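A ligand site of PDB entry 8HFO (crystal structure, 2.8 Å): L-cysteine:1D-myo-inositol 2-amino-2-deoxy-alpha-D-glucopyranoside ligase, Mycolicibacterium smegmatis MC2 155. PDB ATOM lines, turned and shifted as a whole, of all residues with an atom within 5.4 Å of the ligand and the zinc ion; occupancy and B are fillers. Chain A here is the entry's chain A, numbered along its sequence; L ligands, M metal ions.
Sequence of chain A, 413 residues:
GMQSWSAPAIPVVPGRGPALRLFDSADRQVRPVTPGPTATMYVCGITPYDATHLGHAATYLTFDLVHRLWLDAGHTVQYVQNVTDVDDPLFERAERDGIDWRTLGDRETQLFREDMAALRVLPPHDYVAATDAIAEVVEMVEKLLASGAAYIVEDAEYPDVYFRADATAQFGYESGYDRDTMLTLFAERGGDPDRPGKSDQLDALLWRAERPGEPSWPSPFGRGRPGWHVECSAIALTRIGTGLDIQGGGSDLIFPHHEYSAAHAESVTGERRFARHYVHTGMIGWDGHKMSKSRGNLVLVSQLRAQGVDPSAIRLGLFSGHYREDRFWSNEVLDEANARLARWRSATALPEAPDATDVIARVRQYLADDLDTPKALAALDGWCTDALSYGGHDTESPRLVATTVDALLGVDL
S2 of the ligand sits close to ND2 of Asn 82. N2 of the ligand sits close to O of Gly 45. The indole nitrogen of Trp 228 sits close to a sulfur (S2) of the ligand, 3.1 Å away. The backbone NH (N) of Thr 47 is in hydrogen-bond range of an oxygen (O3) of the ligand (3.1 Å). A ring nitrogen (NE2) of His 56 lies within hydrogen-bond range of an oxygen (O3) of the ligand (2.8 Å). OG1 of Thr 84 is in hydrogen-bond range of N2 of the ligand. N2 of the ligand sits at hydrogen-bond distance from OG1 of Thr 47, at 2.7 Å.
OH of Tyr 42 lies close to SG of Cys 232. The side-chain sulfur of Cys 232 sits close to the side-chain amide nitrogen of Asn 82. The indole nitrogen (NE1) of Trp 228 lies close to a ring nitrogen (NE2) of His 257 (3.5 Å). A ring nitrogen (ND1) of His 53 sits close to the backbone NH (N) of Gly 55, at 3.2 Å. A ring nitrogen (ND1) of His 53 is in hydrogen-bond range of the backbone NH (N) of His 56, 3.2 Å away. OH of Tyr 42 sits at hydrogen-bond distance from OD1 of Asn 82 (2.9 Å). The backbone carbonyl oxygen (O) of Gly 45 lies close to the side-chain hydroxyl (OH) of Tyr 60 (3.2 Å). OH of Tyr 60 sits at hydrogen-bond distance from N of Ile 46 (3.4 Å).
Ile 46 touches the ligand. O of Gly 55 touches C13 of the ligand, at 3.8 Å. Thr 59 touches the ligand (OG1 to C13, 3.4 Å). Tyr 60 touches the ligand (OH to C8, 3.3 Å). Gly 250 touches the ligand. Leu 253 touches the ligand (CD1 to O1, 3.97 Å). Thr 281 touches the ligand. CA of Gly 282 touches C12 of the ligand, 3.3 Å away. Met 283 touches the ligand (O to C11, 3.5 Å). Hydrophobic or aromatic side chains that line the ligand: His 56, Tyr 60, Trp 228 and Leu 253. Along chain A the residues within 4 Å of the ligand span positions 44 to 283. The nearest printed residue that does not touch the ligand is Lys 290 (4.1 Å).
Of the 25 residues printed, 3 come within 4 Å of the zinc ion. The nearest printed residue that does not touch the zinc ion is Trp 228 (4.2 Å).
The zinc ion is bound by a sulfur (S2) of the ligand (2.2 Å), a ring nitrogen (NE2) of His 257 (2.3 Å), the side-chain sulfur (SG) of Cys 44 (2.3 Å) and the side-chain sulfur (SG) of Cys 232 (2.3 Å). The zinc ion has four donor atoms within binding distance.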
ATOM      1  N   TYR A  42      10.355 -23.442 -10.092  1.00  0.00           N
ATOM      2  CA  TYR A  42      10.231 -21.987 -10.032  1.00  0.00           C
ATOM      3  C   TYR A  42       9.154 -21.632  -9.017  1.00  0.00           C
ATOM      4  O   TYR A  42       7.999 -22.054  -9.176  1.00  0.00           O
ATOM      5  CB  TYR A  42       9.909 -21.384 -11.391  1.00  0.00           C
ATOM      6  CG  TYR A  42       9.809 -19.867 -11.403  1.00  0.00           C
ATOM      7  CD1 TYR A  42      10.847 -19.095 -11.928  1.00  0.00           C
ATOM      8  CD2 TYR A  42       8.682 -19.201 -10.942  1.00  0.00           C
ATOM      9  CE1 TYR A  42      10.770 -17.721 -11.974  1.00  0.00           C
ATOM     10  CE2 TYR A  42       8.594 -17.817 -10.969  1.00  0.00           C
ATOM     11  CZ  TYR A  42       9.653 -17.079 -11.488  1.00  0.00           C
ATOM     12  OH  TYR A  42       9.594 -15.707 -11.544  1.00  0.00           O
ATOM     13  N   CYS A  44       7.315 -18.394  -7.144  1.00  0.00           N
ATOM     14  CA  CYS A  44       7.117 -16.951  -7.196  1.00  0.00           C
ATOM     15  C   CYS A  44       7.625 -16.319  -5.918  1.00  0.00           C
ATOM     16  O   CYS A  44       7.216 -16.702  -4.810  1.00  0.00           O
ATOM     17  CB  CYS A  44       5.644 -16.641  -7.394  1.00  0.00           C
ATOM     18  SG  CYS A  44       5.124 -16.887  -9.086  1.00  0.00           S
ATOM     19  N   GLY A  45       8.530 -15.340  -6.078  1.00  0.00           N
ATOM     20  CA  GLY A  45       9.217 -14.713  -4.976  1.00  0.00           C
ATOM     21  C   GLY A  45       8.395 -13.633  -4.294  1.00  0.00           C
ATOM     22  O   GLY A  45       7.174 -13.571  -4.401  1.00  0.00           O
ATOM     23  N   ILE A  46       9.091 -12.787  -3.574  1.00  0.00           N
ATOM     24  CA  ILE A  46       8.419 -11.801  -2.746  1.00  0.00           C
ATOM     25  C   ILE A  46       8.266 -10.486  -3.504  1.00  0.00           C
ATOM     26  O   ILE A  46       9.004 -10.185  -4.456  1.00  0.00           O
ATOM     27  CB  ILE A  46       9.161 -11.553  -1.423  1.00  0.00           C
ATOM     28  CG1 ILE A  46      10.559 -11.005  -1.705  1.00  0.00           C
ATOM     29  CG2 ILE A  46       9.253 -12.832  -0.616  1.00  0.00           C
ATOM     30  CD1 ILE A  46      11.141 -10.201  -0.578  1.00  0.00           C
ATOM     31  N   THR A  47       7.306  -9.693  -3.056  1.00  0.00           N
ATOM     32  CA  THR A  47       7.257  -8.283  -3.374  1.00  0.00           C
ATOM     33  C   THR A  47       7.846  -7.546  -2.180  1.00  0.00           C
ATOM     34  O   THR A  47       7.257  -7.575  -1.094  1.00  0.00           O
ATOM     35  CB  THR A  47       5.830  -7.833  -3.644  1.00  0.00           C
ATOM     36  OG1 THR A  47       5.262  -8.688  -4.649  1.00  0.00           O
ATOM     37  CG2 THR A  47       5.795  -6.404  -4.126  1.00  0.00           C
ATOM     38  N   TYR A  49       8.171  -5.789   0.476  1.00  0.00           N
ATOM     39  CA  TYR A  49       7.508  -4.898   1.467  1.00  0.00           C
ATOM     40  C   TYR A  49       6.868  -5.884   2.445  1.00  0.00           C
ATOM     41  O   TYR A  49       6.472  -6.956   1.965  1.00  0.00           O
ATOM     42  CB  TYR A  49       6.562  -3.895   0.809  1.00  0.00           C
ATOM     43  CG  TYR A  49       5.193  -4.389   0.421  1.00  0.00           C
ATOM     44  CD1 TYR A  49       4.978  -4.977  -0.811  1.00  0.00           C
ATOM     45  CD2 TYR A  49       4.111  -4.234   1.259  1.00  0.00           C
ATOM     46  CE1 TYR A  49       3.724  -5.428  -1.186  1.00  0.00           C
ATOM     47  CE2 TYR A  49       2.847  -4.675   0.904  1.00  0.00           C
ATOM     48  CZ  TYR A  49       2.657  -5.277  -0.321  1.00  0.00           C
ATOM     49  OH  TYR A  49       1.416  -5.712  -0.677  1.00  0.00           O
ATOM     50  N   HIS A  53       6.654 -12.188   6.359  1.00  0.00           N
ATOM     51  CA  HIS A  53       5.491 -12.548   7.197  1.00  0.00           C
ATOM     52  C   HIS A  53       5.345 -14.066   7.179  1.00  0.00           C
ATOM     53  O   HIS A  53       6.000 -14.715   6.355  1.00  0.00           O
ATOM     54  CB  HIS A  53       4.230 -11.780   6.807  1.00  0.00           C
ATOM     55  CG  HIS A  53       3.843 -11.770   5.369  1.00  0.00           C
ATOM     56  ND1 HIS A  53       3.371 -12.888   4.717  1.00  0.00           N
ATOM     57  CD2 HIS A  53       3.779 -10.763   4.482  1.00  0.00           C
ATOM     58  CE1 HIS A  53       3.081 -12.582   3.478  1.00  0.00           C
ATOM     59  NE2 HIS A  53       3.315 -11.277   3.302  1.00  0.00           N
ATOM     60  N   GLY A  55       3.099 -15.823   6.058  1.00  0.00           N
ATOM     61  CA  GLY A  55       2.608 -16.304   4.760  1.00  0.00           C
ATOM     62  C   GLY A  55       3.773 -16.578   3.848  1.00  0.00           C
ATOM     63  O   GLY A  55       3.798 -17.653   3.236  1.00  0.00           O
ATOM     64  N   HIS A  56       4.716 -15.641   3.765  1.00  0.00           N
ATOM     65  CA  HIS A  56       5.937 -15.870   2.967  1.00  0.00           C
ATOM     66  C   HIS A  56       6.627 -17.110   3.519  1.00  0.00           C
ATOM     67  O   HIS A  56       6.929 -18.014   2.751  1.00  0.00           O
ATOM     68  CB  HIS A  56       6.927 -14.718   3.177  1.00  0.00           C
ATOM     69  CG  HIS A  56       6.564 -13.440   2.525  1.00  0.00           C
ATOM     70  ND1 HIS A  56       6.809 -12.222   3.118  1.00  0.00           N
ATOM     71  CD2 HIS A  56       6.000 -13.167   1.335  1.00  0.00           C
ATOM     72  CE1 HIS A  56       6.412 -11.262   2.322  1.00  0.00           C
ATOM     73  NE2 HIS A  56       5.899 -11.815   1.230  1.00  0.00           N
ATOM     74  N   THR A  59       5.271 -20.446   2.861  1.00  0.00           N
ATOM     75  CA  THR A  59       5.386 -20.778   1.446  1.00  0.00           C
ATOM     76  C   THR A  59       6.778 -21.310   1.105  1.00  0.00           C
ATOM     77  O   THR A  59       6.900 -22.416   0.574  1.00  0.00           O
ATOM     78  CB  THR A  59       5.048 -19.529   0.594  1.00  0.00           C
ATOM     79  OG1 THR A  59       3.654 -19.255   0.714  1.00  0.00           O
ATOM     80  CG2 THR A  59       5.381 -19.778  -0.878  1.00  0.00           C
ATOM     81  N   TYR A  60       7.830 -20.549   1.405  1.00  0.00           N
ATOM     82  CA  TYR A  60       9.159 -21.005   0.995  1.00  0.00           C
ATOM     83  C   TYR A  60       9.665 -22.158   1.841  1.00  0.00           C
ATOM     84  O   TYR A  60      10.530 -22.915   1.380  1.00  0.00           O
ATOM     85  CB  TYR A  60      10.147 -19.849   1.012  1.00  0.00           C
ATOM     86  CG  TYR A  60       9.625 -18.763   0.130  1.00  0.00           C
ATOM     87  CD1 TYR A  60       9.691 -18.887  -1.249  1.00  0.00           C
ATOM     88  CD2 TYR A  60       9.042 -17.618   0.672  1.00  0.00           C
ATOM     89  CE1 TYR A  60       9.186 -17.908  -2.077  1.00  0.00           C
ATOM     90  CE2 TYR A  60       8.543 -16.641  -0.147  1.00  0.00           C
ATOM     91  CZ  TYR A  60       8.615 -16.787  -1.511  1.00  0.00           C
ATOM     92  OH  TYR A  60       8.118 -15.822  -2.322  1.00  0.00           O
ATOM     93  N   ASN A  82      12.260 -15.251  -7.738  1.00  0.00           N
ATOM     94  CA  ASN A  82      12.364 -13.896  -8.328  1.00  0.00           C
ATOM     95  C   ASN A  82      12.031 -12.845  -7.293  1.00  0.00           C
ATOM     96  O   ASN A  82      11.586 -13.210  -6.210  1.00  0.00           O
ATOM     97  CB  ASN A  82      11.338 -13.700  -9.445  1.00  0.00           C
ATOM     98  CG  ASN A  82       9.914 -13.872  -8.977  1.00  0.00           C
ATOM     99  OD1 ASN A  82       9.479 -15.000  -8.724  1.00  0.00           O
ATOM    100  ND2 ASN A  82       9.171 -12.783  -8.861  1.00  0.00           N
ATOM    101  N   THR A  84       9.837  -9.262  -7.202  1.00  0.00           N
ATOM    102  CA  THR A  84       9.021  -8.258  -7.872  1.00  0.00           C
ATOM    103  C   THR A  84       9.382  -6.895  -7.285  1.00  0.00           C
ATOM    104  O   THR A  84       8.629  -6.289  -6.506  1.00  0.00           O
ATOM    105  CB  THR A  84       7.535  -8.581  -7.715  1.00  0.00           C
ATOM    106  OG1 THR A  84       7.343  -9.996  -7.795  1.00  0.00           O
ATOM    107  CG2 THR A  84       6.724  -7.922  -8.806  1.00  0.00           C
ATOM    108  N   TRP A 228       2.991  -7.835 -14.522  1.00  0.00           N
ATOM    109  CA  TRP A 228       3.306  -8.800 -13.477  1.00  0.00           C
ATOM    110  C   TRP A 228       3.556 -10.196 -14.052  1.00  0.00           C
ATOM    111  O   TRP A 228       4.664 -10.737 -13.947  1.00  0.00           O
ATOM    112  CB  TRP A 228       2.184  -8.816 -12.427  1.00  0.00           C
ATOM    113  CG  TRP A 228       2.481  -9.697 -11.245  1.00  0.00           C
ATOM    114  CD1 TRP A 228       3.710 -10.146 -10.835  1.00  0.00           C
ATOM    115  CD2 TRP A 228       1.534 -10.238 -10.310  1.00  0.00           C
ATOM    116  NE1 TRP A 228       3.578 -10.937  -9.721  1.00  0.00           N
ATOM    117  CE2 TRP A 228       2.254 -11.013  -9.383  1.00  0.00           C
ATOM    118  CE3 TRP A 228       0.140 -10.158 -10.174  1.00  0.00           C
ATOM    119  CZ2 TRP A 228       1.633 -11.674  -8.331  1.00  0.00           C
ATOM    120  CZ3 TRP A 228      -0.464 -10.820  -9.132  1.00  0.00           C
ATOM    121  CH2 TRP A 228       0.267 -11.574  -8.230  1.00  0.00           C
ATOM    122  N   CYS A 232       7.274 -13.201 -14.533  1.00  0.00           N
ATOM    123  CA  CYS A 232       7.593 -14.524 -14.014  1.00  0.00           C
ATOM    124  C   CYS A 232       7.670 -15.582 -15.119  1.00  0.00           C
ATOM    125  O   CYS A 232       8.540 -16.459 -15.064  1.00  0.00           O
ATOM    126  CB  CYS A 232       6.573 -14.922 -12.950  1.00  0.00           C
ATOM    127  SG  CYS A 232       6.818 -14.070 -11.361  1.00  0.00           S
ATOM    128  N   GLY A 249       3.776 -21.156  -5.527  1.00  0.00           N
ATOM    129  CA  GLY A 249       3.650 -19.853  -4.917  1.00  0.00           C
ATOM    130  C   GLY A 249       2.495 -19.829  -3.935  1.00  0.00           C
ATOM    131  O   GLY A 249       1.867 -20.858  -3.656  1.00  0.00           O
ATOM    132  N   GLY A 250       2.231 -18.640  -3.407  1.00  0.00           N
ATOM    133  CA  GLY A 250       1.096 -18.460  -2.525  1.00  0.00           C
ATOM    134  C   GLY A 250      -0.220 -18.768  -3.210  1.00  0.00           C
ATOM    135  O   GLY A 250      -0.313 -18.848  -4.429  1.00  0.00           O
ATOM    136  N   SER A 251      -1.266 -18.921  -2.391  1.00  0.00           N
ATOM    137  CA  SER A 251      -2.528 -19.452  -2.910  1.00  0.00           C
ATOM    138  C   SER A 251      -3.230 -18.466  -3.849  1.00  0.00           C
ATOM    139  O   SER A 251      -3.905 -18.905  -4.780  1.00  0.00           O
ATOM    140  CB  SER A 251      -3.445 -19.822  -1.748  1.00  0.00           C
ATOM    141  OG  SER A 251      -3.364 -18.875  -0.709  1.00  0.00           O
ATOM    142  N   LEU A 253      -2.223 -16.947  -6.232  1.00  0.00           N
ATOM    143  CA  LEU A 253      -1.635 -16.951  -7.562  1.00  0.00           C
ATOM    144  C   LEU A 253      -2.214 -18.024  -8.481  1.00  0.00           C
ATOM    145  O   LEU A 253      -1.897 -18.026  -9.678  1.00  0.00           O
ATOM    146  CB  LEU A 253      -0.114 -17.101  -7.433  1.00  0.00           C
ATOM    147  CG  LEU A 253       0.703 -15.867  -6.993  1.00  0.00           C
ATOM    148  CD1 LEU A 253       0.011 -15.006  -5.945  1.00  0.00           C
ATOM    149  CD2 LEU A 253       2.073 -16.308  -6.451  1.00  0.00           C
ATOM    150  N   HIS A 257      -2.444 -14.942 -11.498  1.00  0.00           N
ATOM    151  CA  HIS A 257      -1.023 -14.923 -11.816  1.00  0.00           C
ATOM    152  C   HIS A 257      -0.570 -16.140 -12.620  1.00  0.00           C
ATOM    153  O   HIS A 257      -0.126 -16.004 -13.761  1.00  0.00           O
ATOM    154  CB  HIS A 257      -0.221 -14.813 -10.523  1.00  0.00           C
ATOM    155  CG  HIS A 257       1.202 -14.435 -10.764  1.00  0.00           C
ATOM    156  ND1 HIS A 257       1.563 -13.555 -11.770  1.00  0.00           N
ATOM    157  CD2 HIS A 257       2.359 -14.854 -10.198  1.00  0.00           C
ATOM    158  CE1 HIS A 257       2.877 -13.419 -11.785  1.00  0.00           C
ATOM    159  NE2 HIS A 257       3.383 -14.203 -10.848  1.00  0.00           N
ATOM    160  N   HIS A 258      -0.701 -17.338 -12.048  1.00  0.00           N
ATOM    161  CA  HIS A 258      -0.105 -18.530 -12.661  1.00  0.00           C
ATOM    162  C   HIS A 258      -0.838 -18.936 -13.934  1.00  0.00           C
ATOM    163  O   HIS A 258      -0.209 -19.430 -14.880  1.00  0.00           O
ATOM    164  CB  HIS A 258      -0.085 -19.671 -11.658  1.00  0.00           C
ATOM    165  CG  HIS A 258       0.920 -19.487 -10.553  1.00  0.00           C
ATOM    166  ND1 HIS A 258       0.943 -20.282  -9.429  1.00  0.00           N
ATOM    167  CD2 HIS A 258       1.930 -18.606 -10.418  1.00  0.00           C
ATOM    168  CE1 HIS A 258       1.927 -19.890  -8.635  1.00  0.00           C
ATOM    169  NE2 HIS A 258       2.547 -18.868  -9.220  1.00  0.00           N
ATOM    170  N   THR A 281       0.114 -22.690  -1.690  1.00  0.00           N
ATOM    171  CA  THR A 281       0.166 -22.853  -0.246  1.00  0.00           C
ATOM    172  C   THR A 281       0.107 -21.468   0.363  1.00  0.00           C
ATOM    173  O   THR A 281       0.474 -20.484  -0.276  1.00  0.00           O
ATOM    174  CB  THR A 281       1.445 -23.576   0.187  1.00  0.00           C
ATOM    175  OG1 THR A 281       1.389 -23.881   1.587  1.00  0.00           O
ATOM    176  CG2 THR A 281       2.673 -22.706  -0.115  1.00  0.00           C
ATOM    177  N   GLY A 282      -0.360 -21.385   1.607  1.00  0.00           N
ATOM    178  CA  GLY A 282      -0.369 -20.091   2.243  1.00  0.00           C
ATOM    179  C   GLY A 282      -0.907 -20.019   3.649  1.00  0.00           C
ATOM    180  O   GLY A 282      -1.717 -20.849   4.078  1.00  0.00           O
ATOM    181  N   MET A 283      -0.453 -19.005   4.374  1.00  0.00           N
ATOM    182  CA  MET A 283      -0.951 -18.669   5.695  1.00  0.00           C
ATOM    183  C   MET A 283      -1.854 -17.450   5.596  1.00  0.00           C
ATOM    184  O   MET A 283      -1.752 -16.657   4.658  1.00  0.00           O
ATOM    185  CB  MET A 283       0.214 -18.378   6.652  1.00  0.00           C
ATOM    186  CG  MET A 283       0.491 -19.477   7.674  1.00  0.00           C
ATOM    187  SD  MET A 283      -0.511 -19.310   9.157  1.00  0.00           S
ATOM    188  CE  MET A 283      -0.186 -17.606   9.588  1.00  0.00           C
ATOM    189  N   LYS A 290      -5.293 -11.840   3.836  1.00  0.00           N
ATOM    190  CA  LYS A 290      -3.853 -11.903   3.633  1.00  0.00           C
ATOM    191  C   LYS A 290      -3.152 -10.975   4.614  1.00  0.00           C
ATOM    192  O   LYS A 290      -3.683  -9.928   4.999  1.00  0.00           O
ATOM    193  CB  LYS A 290      -3.508 -11.536   2.180  1.00  0.00           C
ATOM    194  CG  LYS A 290      -2.034 -11.265   1.907  1.00  0.00           C
HETATM  195  N1  LIG L   1       4.569 -11.426  -3.615  1.00  0.00           N
HETATM  196  C1  LIG L   1       3.934 -13.179  -1.591  1.00  0.00           C
HETATM  197  C2  LIG L   1       2.839 -13.632  -0.862  1.00  0.00           C
HETATM  198  C3  LIG L   1       2.798 -14.955  -0.436  1.00  0.00           C
HETATM  199  C4  LIG L   1       3.863 -15.806  -0.721  1.00  0.00           C
HETATM  200  C5  LIG L   1       3.915 -12.001  -4.669  1.00  0.00           C
HETATM  201  C6  LIG L   1       4.564 -11.830  -6.027  1.00  0.00           C
HETATM  202  C7  LIG L   1       4.832 -13.172  -6.684  1.00  0.00           C
HETATM  203  C8  LIG L   1       4.942 -15.339  -1.463  1.00  0.00           C
HETATM  204  N2  LIG L   1       5.778 -10.996  -5.951  1.00  0.00           N
HETATM  205  O1  LIG L   1       2.851 -12.609  -4.540  1.00  0.00           O
HETATM  206  C9  LIG L   1       4.980 -14.035  -1.912  1.00  0.00           C
HETATM  207  C10 LIG L   1       1.603 -15.492   0.254  1.00  0.00           C
HETATM  208  C11 LIG L   1      -0.543 -15.769   1.455  1.00  0.00           C
HETATM  209  C12 LIG L   1       0.034 -16.953   1.184  1.00  0.00           C
HETATM  210  C13 LIG L   1       1.266 -16.807   0.495  1.00  0.00           C
HETATM  211  O2  LIG L   1       2.713 -10.939  -2.085  1.00  0.00           O
HETATM  212  O3  LIG L   1       5.037 -10.856  -1.250  1.00  0.00           O
HETATM  213  S1  LIG L   1       0.381 -14.469   0.888  1.00  0.00           S
HETATM  214  S2  LIG L   1       5.462 -13.044  -8.382  1.00  0.00           S
HETATM  215  S3  LIG L   1       4.040 -11.478  -2.062  1.00  0.00           S
HETATM  216 ZN    ZN M   1       5.307 -14.753  -9.817  1.00  0.00          ZN
